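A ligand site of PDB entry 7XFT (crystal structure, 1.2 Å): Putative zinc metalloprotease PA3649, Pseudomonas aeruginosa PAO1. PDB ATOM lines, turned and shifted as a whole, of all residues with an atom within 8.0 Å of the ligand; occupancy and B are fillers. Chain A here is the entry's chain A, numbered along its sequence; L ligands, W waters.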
ATOM      1  N   LEU A   7      16.106  -7.893  11.290  1.00  0.00           N
ATOM      2  CA  LEU A   7      15.536  -7.766  12.630  1.00  0.00           C
ATOM      3  C   LEU A   7      15.272  -9.113  13.264  1.00  0.00           C
ATOM      4  O   LEU A   7      14.605  -9.967  12.677  1.00  0.00           O
ATOM      5  CB  LEU A   7      14.239  -6.956  12.557  1.00  0.00           C
ATOM      6  CG  LEU A   7      14.329  -5.623  11.823  1.00  0.00           C
ATOM      7  CD1 LEU A   7      12.976  -4.900  11.919  1.00  0.00           C
ATOM      8  CD2 LEU A   7      15.440  -4.745  12.339  1.00  0.00           C
ATOM      9  N   GLU A   9      14.725  -9.193  17.007  1.00  0.00           N
ATOM     10  CA  GLU A   9      14.032  -8.915  18.257  1.00  0.00           C
ATOM     11  C   GLU A   9      13.410  -7.546  18.112  1.00  0.00           C
ATOM     12  O   GLU A   9      13.960  -6.675  17.447  1.00  0.00           O
ATOM     13  CB  GLU A   9      15.013  -8.932  19.431  1.00  0.00           C
ATOM     14  CG  GLU A   9      14.360  -9.056  20.796  1.00  0.00           C
ATOM     15  CD  GLU A   9      15.281  -9.744  21.801  1.00  0.00           C
ATOM     16  OE1 GLU A   9      16.253  -9.102  22.249  1.00  0.00           O
ATOM     17  OE2 GLU A   9      15.048 -10.926  22.138  1.00  0.00           O
ATOM     18  N   LEU A  10      12.261  -7.363  18.744  1.00  0.00           N
ATOM     19  CA  LEU A  10      11.542  -6.106  18.676  1.00  0.00           C
ATOM     20  C   LEU A  10      10.986  -5.746  20.050  1.00  0.00           C
ATOM     21  O   LEU A  10      10.374  -6.585  20.715  1.00  0.00           O
ATOM     22  CB  LEU A  10      10.335  -6.198  17.725  1.00  0.00           C
ATOM     23  CG  LEU A  10      10.622  -6.178  16.228  1.00  0.00           C
ATOM     24  CD1 LEU A  10       9.394  -6.642  15.452  1.00  0.00           C
ATOM     25  CD2 LEU A  10      10.983  -4.785  15.819  1.00  0.00           C
ATOM     26  N   ASP A  11      11.151  -4.491  20.435  1.00  0.00           N
ATOM     27  CA  ASP A  11      10.527  -3.952  21.650  1.00  0.00           C
ATOM     28  C   ASP A  11       9.050  -3.733  21.378  1.00  0.00           C
ATOM     29  O   ASP A  11       8.702  -2.944  20.497  1.00  0.00           O
ATOM     30  CB  ASP A  11      11.224  -2.618  21.962  1.00  0.00           C
ATOM     31  CG  ASP A  11      10.605  -1.855  23.132  1.00  0.00           C
ATOM     32  OD1 ASP A  11       9.577  -2.301  23.671  1.00  0.00           O
ATOM     33  OD2 ASP A  11      11.157  -0.774  23.451  1.00  0.00           O
ATOM     34  N   GLY A  14       8.239  -0.118  21.306  1.00  0.00           N
ATOM     35  CA  GLY A  14       9.202   0.722  20.636  1.00  0.00           C
ATOM     36  C   GLY A  14       8.800   1.159  19.247  1.00  0.00           C
ATOM     37  O   GLY A  14       7.781   0.730  18.688  1.00  0.00           O
ATOM     38  N   PRO A  15       9.640   2.024  18.657  1.00  0.00           N
ATOM     39  CA  PRO A  15       9.307   2.613  17.361  1.00  0.00           C
ATOM     40  C   PRO A  15       9.196   1.603  16.236  1.00  0.00           C
ATOM     41  O   PRO A  15       8.355   1.781  15.355  1.00  0.00           O
ATOM     42  CB  PRO A  15      10.464   3.604  17.146  1.00  0.00           C
ATOM     43  CG  PRO A  15      10.899   3.999  18.508  1.00  0.00           C
ATOM     44  CD  PRO A  15      10.744   2.734  19.328  1.00  0.00           C
ATOM     45  N   ALA A  16      10.046   0.577  16.211  1.00  0.00           N
ATOM     46  CA  ALA A  16      10.041  -0.352  15.086  1.00  0.00           C
ATOM     47  C   ALA A  16       8.724  -1.108  15.006  1.00  0.00           C
ATOM     48  O   ALA A  16       8.122  -1.230  13.942  1.00  0.00           O
ATOM     49  CB  ALA A  16      11.230  -1.289  15.194  1.00  0.00           C
ATOM     50  N   TRP A  38      24.376  -4.625  10.002  1.00  0.00           N
ATOM     51  CA  TRP A  38      23.599  -4.207  11.155  1.00  0.00           C
ATOM     52  C   TRP A  38      24.289  -3.056  11.897  1.00  0.00           C
ATOM     53  O   TRP A  38      23.621  -2.147  12.384  1.00  0.00           O
ATOM     54  CB  TRP A  38      23.371  -5.406  12.071  1.00  0.00           C
ATOM     55  CG  TRP A  38      22.683  -5.030  13.341  1.00  0.00           C
ATOM     56  CD1 TRP A  38      23.202  -5.050  14.593  1.00  0.00           C
ATOM     57  CD2 TRP A  38      21.340  -4.575  13.474  1.00  0.00           C
ATOM     58  NE1 TRP A  38      22.272  -4.615  15.507  1.00  0.00           N
ATOM     59  CE2 TRP A  38      21.112  -4.330  14.851  1.00  0.00           C
ATOM     60  CE3 TRP A  38      20.295  -4.348  12.567  1.00  0.00           C
ATOM     61  CZ2 TRP A  38      19.903  -3.862  15.329  1.00  0.00           C
ATOM     62  CZ3 TRP A  38      19.093  -3.885  13.050  1.00  0.00           C
ATOM     63  CH2 TRP A  38      18.897  -3.658  14.422  1.00  0.00           C
ATOM     64  N   GLN A  39      25.614  -3.089  11.993  1.00  0.00           N
ATOM     65  CA  GLN A  39      26.306  -2.029  12.713  1.00  0.00           C
ATOM     66  C   GLN A  39      26.042  -0.670  12.083  1.00  0.00           C
ATOM     67  O   GLN A  39      25.961   0.338  12.793  1.00  0.00           O
ATOM     68  CB  GLN A  39      27.806  -2.303  12.787  1.00  0.00           C
ATOM     69  CG  GLN A  39      28.526  -1.288  13.666  1.00  0.00           C
ATOM     70  CD  GLN A  39      28.142  -1.407  15.128  1.00  0.00           C
ATOM     71  OE1 GLN A  39      27.853  -0.408  15.795  1.00  0.00           O
ATOM     72  NE2 GLN A  39      28.158  -2.627  15.648  1.00  0.00           N
ATOM     73  N   GLN A  40      25.897  -0.614  10.769  1.00  0.00           N
ATOM     74  CA  GLN A  40      25.538   0.650  10.126  1.00  0.00           C
ATOM     75  C   GLN A  40      24.164   1.131  10.585  1.00  0.00           C
ATOM     76  O   GLN A  40      23.945   2.323  10.765  1.00  0.00           O
ATOM     77  CB  GLN A  40      25.601   0.515   8.610  1.00  0.00           C
ATOM     78  CG  GLN A  40      27.036   0.629   8.069  1.00  0.00           C
ATOM     79  CD  GLN A  40      27.112   0.554   6.560  1.00  0.00           C
ATOM     80  OE1 GLN A  40      26.097   0.664   5.874  1.00  0.00           O
ATOM     81  NE2 GLN A  40      28.321   0.384   6.044  1.00  0.00           N
ATOM     82  N   VAL A  41      23.224   0.206  10.771  1.00  0.00           N
ATOM     83  CA  VAL A  41      21.917   0.575  11.319  1.00  0.00           C
ATOM     84  C   VAL A  41      22.080   1.154  12.717  1.00  0.00           C
ATOM     85  O   VAL A  41      21.560   2.230  13.033  1.00  0.00           O
ATOM     86  CB  VAL A  41      20.969  -0.640  11.315  1.00  0.00           C
ATOM     87  CG1 VAL A  41      19.619  -0.240  11.940  1.00  0.00           C
ATOM     88  CG2 VAL A  41      20.789  -1.216   9.923  1.00  0.00           C
ATOM     89  N   VAL A  42      22.801   0.441  13.585  1.00  0.00           N
ATOM     90  CA  VAL A  42      23.005   0.905  14.961  1.00  0.00           C
ATOM     91  C   VAL A  42      23.609   2.296  14.972  1.00  0.00           C
ATOM     92  O   VAL A  42      23.160   3.193  15.692  1.00  0.00           O
ATOM     93  CB  VAL A  42      23.897  -0.077  15.739  1.00  0.00           C
ATOM     94  CG1 VAL A  42      24.260   0.496  17.093  1.00  0.00           C
ATOM     95  CG2 VAL A  42      23.217  -1.428  15.883  1.00  0.00           C
ATOM     96  N   ASP A  43      24.657   2.506  14.177  1.00  0.00           N
ATOM     97  CA  ASP A  43      25.350   3.790  14.211  1.00  0.00           C
ATOM     98  C   ASP A  43      24.436   4.904  13.719  1.00  0.00           C
ATOM     99  O   ASP A  43      24.441   6.011  14.251  1.00  0.00           O
ATOM    100  CB  ASP A  43      26.588   3.711  13.318  1.00  0.00           C
ATOM    101  CG  ASP A  43      27.720   2.897  13.938  1.00  0.00           C
ATOM    102  OD1 ASP A  43      27.631   2.511  15.112  1.00  0.00           O
ATOM    103  OD2 ASP A  43      28.702   2.641  13.215  1.00  0.00           O
ATOM    104  N   SER A  44      23.657   4.622  12.688  1.00  0.00           N
ATOM    105  CA  SER A  44      22.806   5.660  12.125  1.00  0.00           C
ATOM    106  C   SER A  44      21.632   5.967  13.058  1.00  0.00           C
ATOM    107  O   SER A  44      21.260   7.132  13.219  1.00  0.00           O
ATOM    108  CB  SER A  44      22.314   5.192  10.761  1.00  0.00           C
ATOM    109  OG  SER A  44      23.359   5.342   9.822  1.00  0.00           O
ATOM    110  N   VAL A  45      21.035   4.944  13.660  1.00  0.00           N
ATOM    111  CA  VAL A  45      19.936   5.168  14.600  1.00  0.00           C
ATOM    112  C   VAL A  45      20.432   5.932  15.811  1.00  0.00           C
ATOM    113  O   VAL A  45      19.806   6.904  16.267  1.00  0.00           O
ATOM    114  CB  VAL A  45      19.318   3.807  14.999  1.00  0.00           C
ATOM    115  CG1 VAL A  45      18.462   3.943  16.240  1.00  0.00           C
ATOM    116  CG2 VAL A  45      18.550   3.247  13.847  1.00  0.00           C
ATOM    117  N   ARG A  46      21.562   5.512  16.378  1.00  0.00           N
ATOM    118  CA  ARG A  46      22.027   6.165  17.592  1.00  0.00           C
ATOM    119  C   ARG A  46      22.284   7.636  17.380  1.00  0.00           C
ATOM    120  O   ARG A  46      22.075   8.447  18.283  1.00  0.00           O
ATOM    121  CB  ARG A  46      23.308   5.501  18.084  1.00  0.00           C
ATOM    122  CG  ARG A  46      23.040   4.200  18.774  1.00  0.00           C
ATOM    123  CD  ARG A  46      24.322   3.520  19.205  1.00  0.00           C
ATOM    124  NE  ARG A  46      25.063   4.302  20.188  1.00  0.00           N
ATOM    125  CZ  ARG A  46      24.807   4.329  21.483  1.00  0.00           C
ATOM    126  NH1 ARG A  46      23.846   3.593  22.018  1.00  0.00           N
ATOM    127  NH2 ARG A  46      25.532   5.120  22.270  1.00  0.00           N
ATOM    128  N   ALA A  47      22.745   8.011  16.179  1.00  0.00           N
ATOM    129  CA  ALA A  47      23.065   9.402  15.888  1.00  0.00           C
ATOM    130  C   ALA A  47      21.852  10.270  15.634  1.00  0.00           C
ATOM    131  O   ALA A  47      22.008  11.488  15.490  1.00  0.00           O
ATOM    132  CB  ALA A  47      23.957   9.442  14.647  1.00  0.00           C
ATOM    133  N   LEU A  68       9.949   5.468  10.021  1.00  0.00           N
ATOM    134  CA  LEU A  68      10.345   5.054  11.361  1.00  0.00           C
ATOM    135  C   LEU A  68      10.633   6.298  12.182  1.00  0.00           C
ATOM    136  O   LEU A  68      11.521   7.081  11.847  1.00  0.00           O
ATOM    137  CB  LEU A  68      11.572   4.153  11.309  1.00  0.00           C
ATOM    138  CG  LEU A  68      12.186   3.710  12.634  1.00  0.00           C
ATOM    139  CD1 LEU A  68      11.230   2.887  13.460  1.00  0.00           C
ATOM    140  CD2 LEU A  68      13.498   2.959  12.378  1.00  0.00           C
ATOM    141  N   LEU A  70      12.242   7.660  15.195  1.00  0.00           N
ATOM    142  CA  LEU A  70      13.179   7.247  16.237  1.00  0.00           C
ATOM    143  C   LEU A  70      12.893   7.963  17.539  1.00  0.00           C
ATOM    144  O   LEU A  70      12.605   9.169  17.564  1.00  0.00           O
ATOM    145  CB  LEU A  70      14.616   7.522  15.788  1.00  0.00           C
ATOM    146  CG  LEU A  70      15.090   6.743  14.561  1.00  0.00           C
ATOM    147  CD1 LEU A  70      16.491   7.144  14.141  1.00  0.00           C
ATOM    148  CD2 LEU A  70      14.986   5.233  14.802  1.00  0.00           C
ATOM    149  N   ALA A  71      12.992   7.223  18.626  1.00  0.00           N
ATOM    150  CA  ALA A  71      12.840   7.774  19.947  1.00  0.00           C
ATOM    151  C   ALA A  71      14.194   8.161  20.497  1.00  0.00           C
ATOM    152  O   ALA A  71      15.197   8.208  19.773  1.00  0.00           O
ATOM    153  CB  ALA A  71      12.111   6.778  20.835  1.00  0.00           C
ATOM    154  N   ARG A  73      16.817   7.589  23.956  1.00  0.00           N
ATOM    155  CA  ARG A  73      17.112   6.829  25.155  1.00  0.00           C
ATOM    156  C   ARG A  73      18.500   7.195  25.633  1.00  0.00           C
ATOM    157  O   ARG A  73      19.374   7.514  24.836  1.00  0.00           O
ATOM    158  CB  ARG A  73      17.037   5.325  24.902  1.00  0.00           C
ATOM    159  CG  ARG A  73      15.637   4.822  24.620  1.00  0.00           C
ATOM    160  CD  ARG A  73      15.134   3.974  25.787  1.00  0.00           C
ATOM    161  NE  ARG A  73      13.889   3.274  25.477  1.00  0.00           N
ATOM    162  CZ  ARG A  73      13.665   1.980  25.676  1.00  0.00           C
ATOM    163  NH1 ARG A  73      14.620   1.174  26.101  1.00  0.00           N
ATOM    164  NH2 ARG A  73      12.453   1.489  25.430  1.00  0.00           N
ATOM    165  N   SER A  80      20.871   8.880  22.885  1.00  0.00           N
ATOM    166  CA  SER A  80      20.975   8.342  21.543  1.00  0.00           C
ATOM    167  C   SER A  80      19.591   8.130  20.964  1.00  0.00           C
ATOM    168  O   SER A  80      18.599   8.002  21.686  1.00  0.00           O
ATOM    169  CB  SER A  80      21.656   6.968  21.556  1.00  0.00           C
ATOM    170  OG  SER A  80      22.942   6.989  22.125  1.00  0.00           O
ATOM    171  N   GLY A  81      19.543   8.019  19.635  1.00  0.00           N
ATOM    172  CA  GLY A  81      18.329   7.547  18.996  1.00  0.00           C
ATOM    173  C   GLY A  81      18.068   6.099  19.345  1.00  0.00           C
ATOM    174  O   GLY A  81      18.977   5.333  19.632  1.00  0.00           O
ATOM    175  N   TYR A  82      16.797   5.720  19.268  1.00  0.00           N
ATOM    176  CA  TYR A  82      16.341   4.402  19.669  1.00  0.00           C
ATOM    177  C   TYR A  82      15.264   3.930  18.708  1.00  0.00           C
ATOM    178  O   TYR A  82      14.281   4.627  18.471  1.00  0.00           O
ATOM    179  CB  TYR A  82      15.735   4.442  21.090  1.00  0.00           C
ATOM    180  CG  TYR A  82      15.192   3.117  21.586  1.00  0.00           C
ATOM    181  CD1 TYR A  82      16.047   2.093  21.932  1.00  0.00           C
ATOM    182  CD2 TYR A  82      13.828   2.916  21.762  1.00  0.00           C
ATOM    183  CE1 TYR A  82      15.565   0.903  22.410  1.00  0.00           C
ATOM    184  CE2 TYR A  82      13.333   1.703  22.213  1.00  0.00           C
ATOM    185  CZ  TYR A  82      14.221   0.716  22.550  1.00  0.00           C
ATOM    186  OH  TYR A  82      13.778  -0.486  23.022  1.00  0.00           O
ATOM    187  N   MET A  83      15.458   2.727  18.155  1.00  0.00           N
ATOM    188  CA  MET A  83      14.468   2.124  17.276  1.00  0.00           C
ATOM    189  C   MET A  83      13.703   0.968  17.887  1.00  0.00           C
ATOM    190  O   MET A  83      12.653   0.619  17.359  1.00  0.00           O
ATOM    191  CB  MET A  83      15.102   1.700  15.946  1.00  0.00           C
ATOM    192  CG  MET A  83      15.556   0.322  15.803  1.00  0.00           C
ATOM    193  SD  MET A  83      16.205  -0.042  14.144  1.00  0.00           S
ATOM    194  CE  MET A  83      14.776  -0.673  13.280  1.00  0.00           C
ATOM    195  N   GLY A  84      14.192   0.388  18.968  1.00  0.00           N
ATOM    196  CA  GLY A  84      13.531  -0.745  19.562  1.00  0.00           C
ATOM    197  C   GLY A  84      13.628  -2.027  18.767  1.00  0.00           C
ATOM    198  O   GLY A  84      12.619  -2.741  18.625  1.00  0.00           O
ATOM    199  N   ALA A  85      14.810  -2.337  18.257  1.00  0.00           N
ATOM    200  CA  ALA A  85      15.030  -3.601  17.557  1.00  0.00           C
ATOM    201  C   ALA A  85      16.458  -4.080  17.775  1.00  0.00           C
ATOM    202  O   ALA A  85      17.374  -3.285  17.998  1.00  0.00           O
ATOM    203  CB  ALA A  85      14.772  -3.482  16.061  1.00  0.00           C
ATOM    204  N   GLY A  86      16.637  -5.390  17.645  1.00  0.00           N
ATOM    205  CA  GLY A  86      17.932  -6.026  17.731  1.00  0.00           C
ATOM    206  C   GLY A  86      18.192  -7.025  16.604  1.00  0.00           C
ATOM    207  O   GLY A  86      17.263  -7.460  15.910  1.00  0.00           O
HETATM  208  N1  LIG L   1      19.303  -1.758  19.484  1.00  0.00           N
HETATM  209  C1  LIG L   1      19.303  -0.318  19.295  1.00  0.00           C
HETATM  210  C2  LIG L   1      17.897   0.251  19.188  1.00  0.00           C
HETATM  211  O1  LIG L   1      17.807   1.428  18.831  1.00  0.00           O
HETATM  212  C3  LIG L   1      20.158   0.097  18.071  1.00  0.00           C
HETATM  213  C4  LIG L   1      19.421  -0.093  16.771  1.00  0.00           C
HETATM  214  C5  LIG L   1      20.519   1.550  18.189  1.00  0.00           C
HETATM  215  O2  LIG L   1      16.886  -0.431  19.460  1.00  0.00           O
HETATM  216  O   HOH W   1      16.421  -2.272  21.245  1.00  0.00           O
HETATM  217  O   HOH W   2      21.997   2.032  20.586  1.00  0.00           O
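OD2 of Asp 11 is in hydrogen-bond range of OH of Tyr 82 (2.7 Å). The backbone carbonyl oxygen (O) of Met 83 sits at hydrogen-bond distance from the backbone NH (N) of Ala 16 (2.8 Å). The backbone carbonyl oxygen (O) of Tyr 82 is in hydrogen-bond range of the backbone NH (N) of Ala 71 (2.9 Å). OG of Ser 80 lies within hydrogen-bond range of NH2 of Arg 46 (3.2 Å). The backbone carbonyl oxygen of Arg 46 is in hydrogen-bond range of the backbone NH of Gly 81 (2.9 Å). N of Asp 11 is in hydrogen-bond range of O of Gly 84 (2.9 Å). The side-chain hydroxyl of Tyr 82 sits close to the guanidinium group of Arg 73, at 3.4 Å.
Val 42 touches the ligand (O to C5, 3.99 Å). CG1 of Val 45 touches O1 of the ligand, 3.7 Å away. Arg 46 touches the ligand. Tyr 82 touches the ligand (CA to O1, 3.4 Å). Hydrophobic or aromatic side chains that line the ligand: Val 45, Tyr 82 and Met 83. Of the 28 residues printed, 7 come within 4 Å of the ligand.
N of Gly 84 sits at hydrogen-bond distance from O2 of the ligand, at 2.9 Å. The backbone NH of Ala 85 lies within hydrogen-bond range of an oxygen (O2) of the ligand, at 3.1 Å. O of Ala 85 sits at hydrogen-bond distance from N1 of the ligand, at 2.9 Å. An oxygen (O1) of the ligand is in hydrogen-bond range of the backbone NH of Met 83, at 2.8 Å.
Water W1 bridges an oxygen (O2) of the ligand (2.6 Å) and the backbone NH of Ala 85 (3.4 Å).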
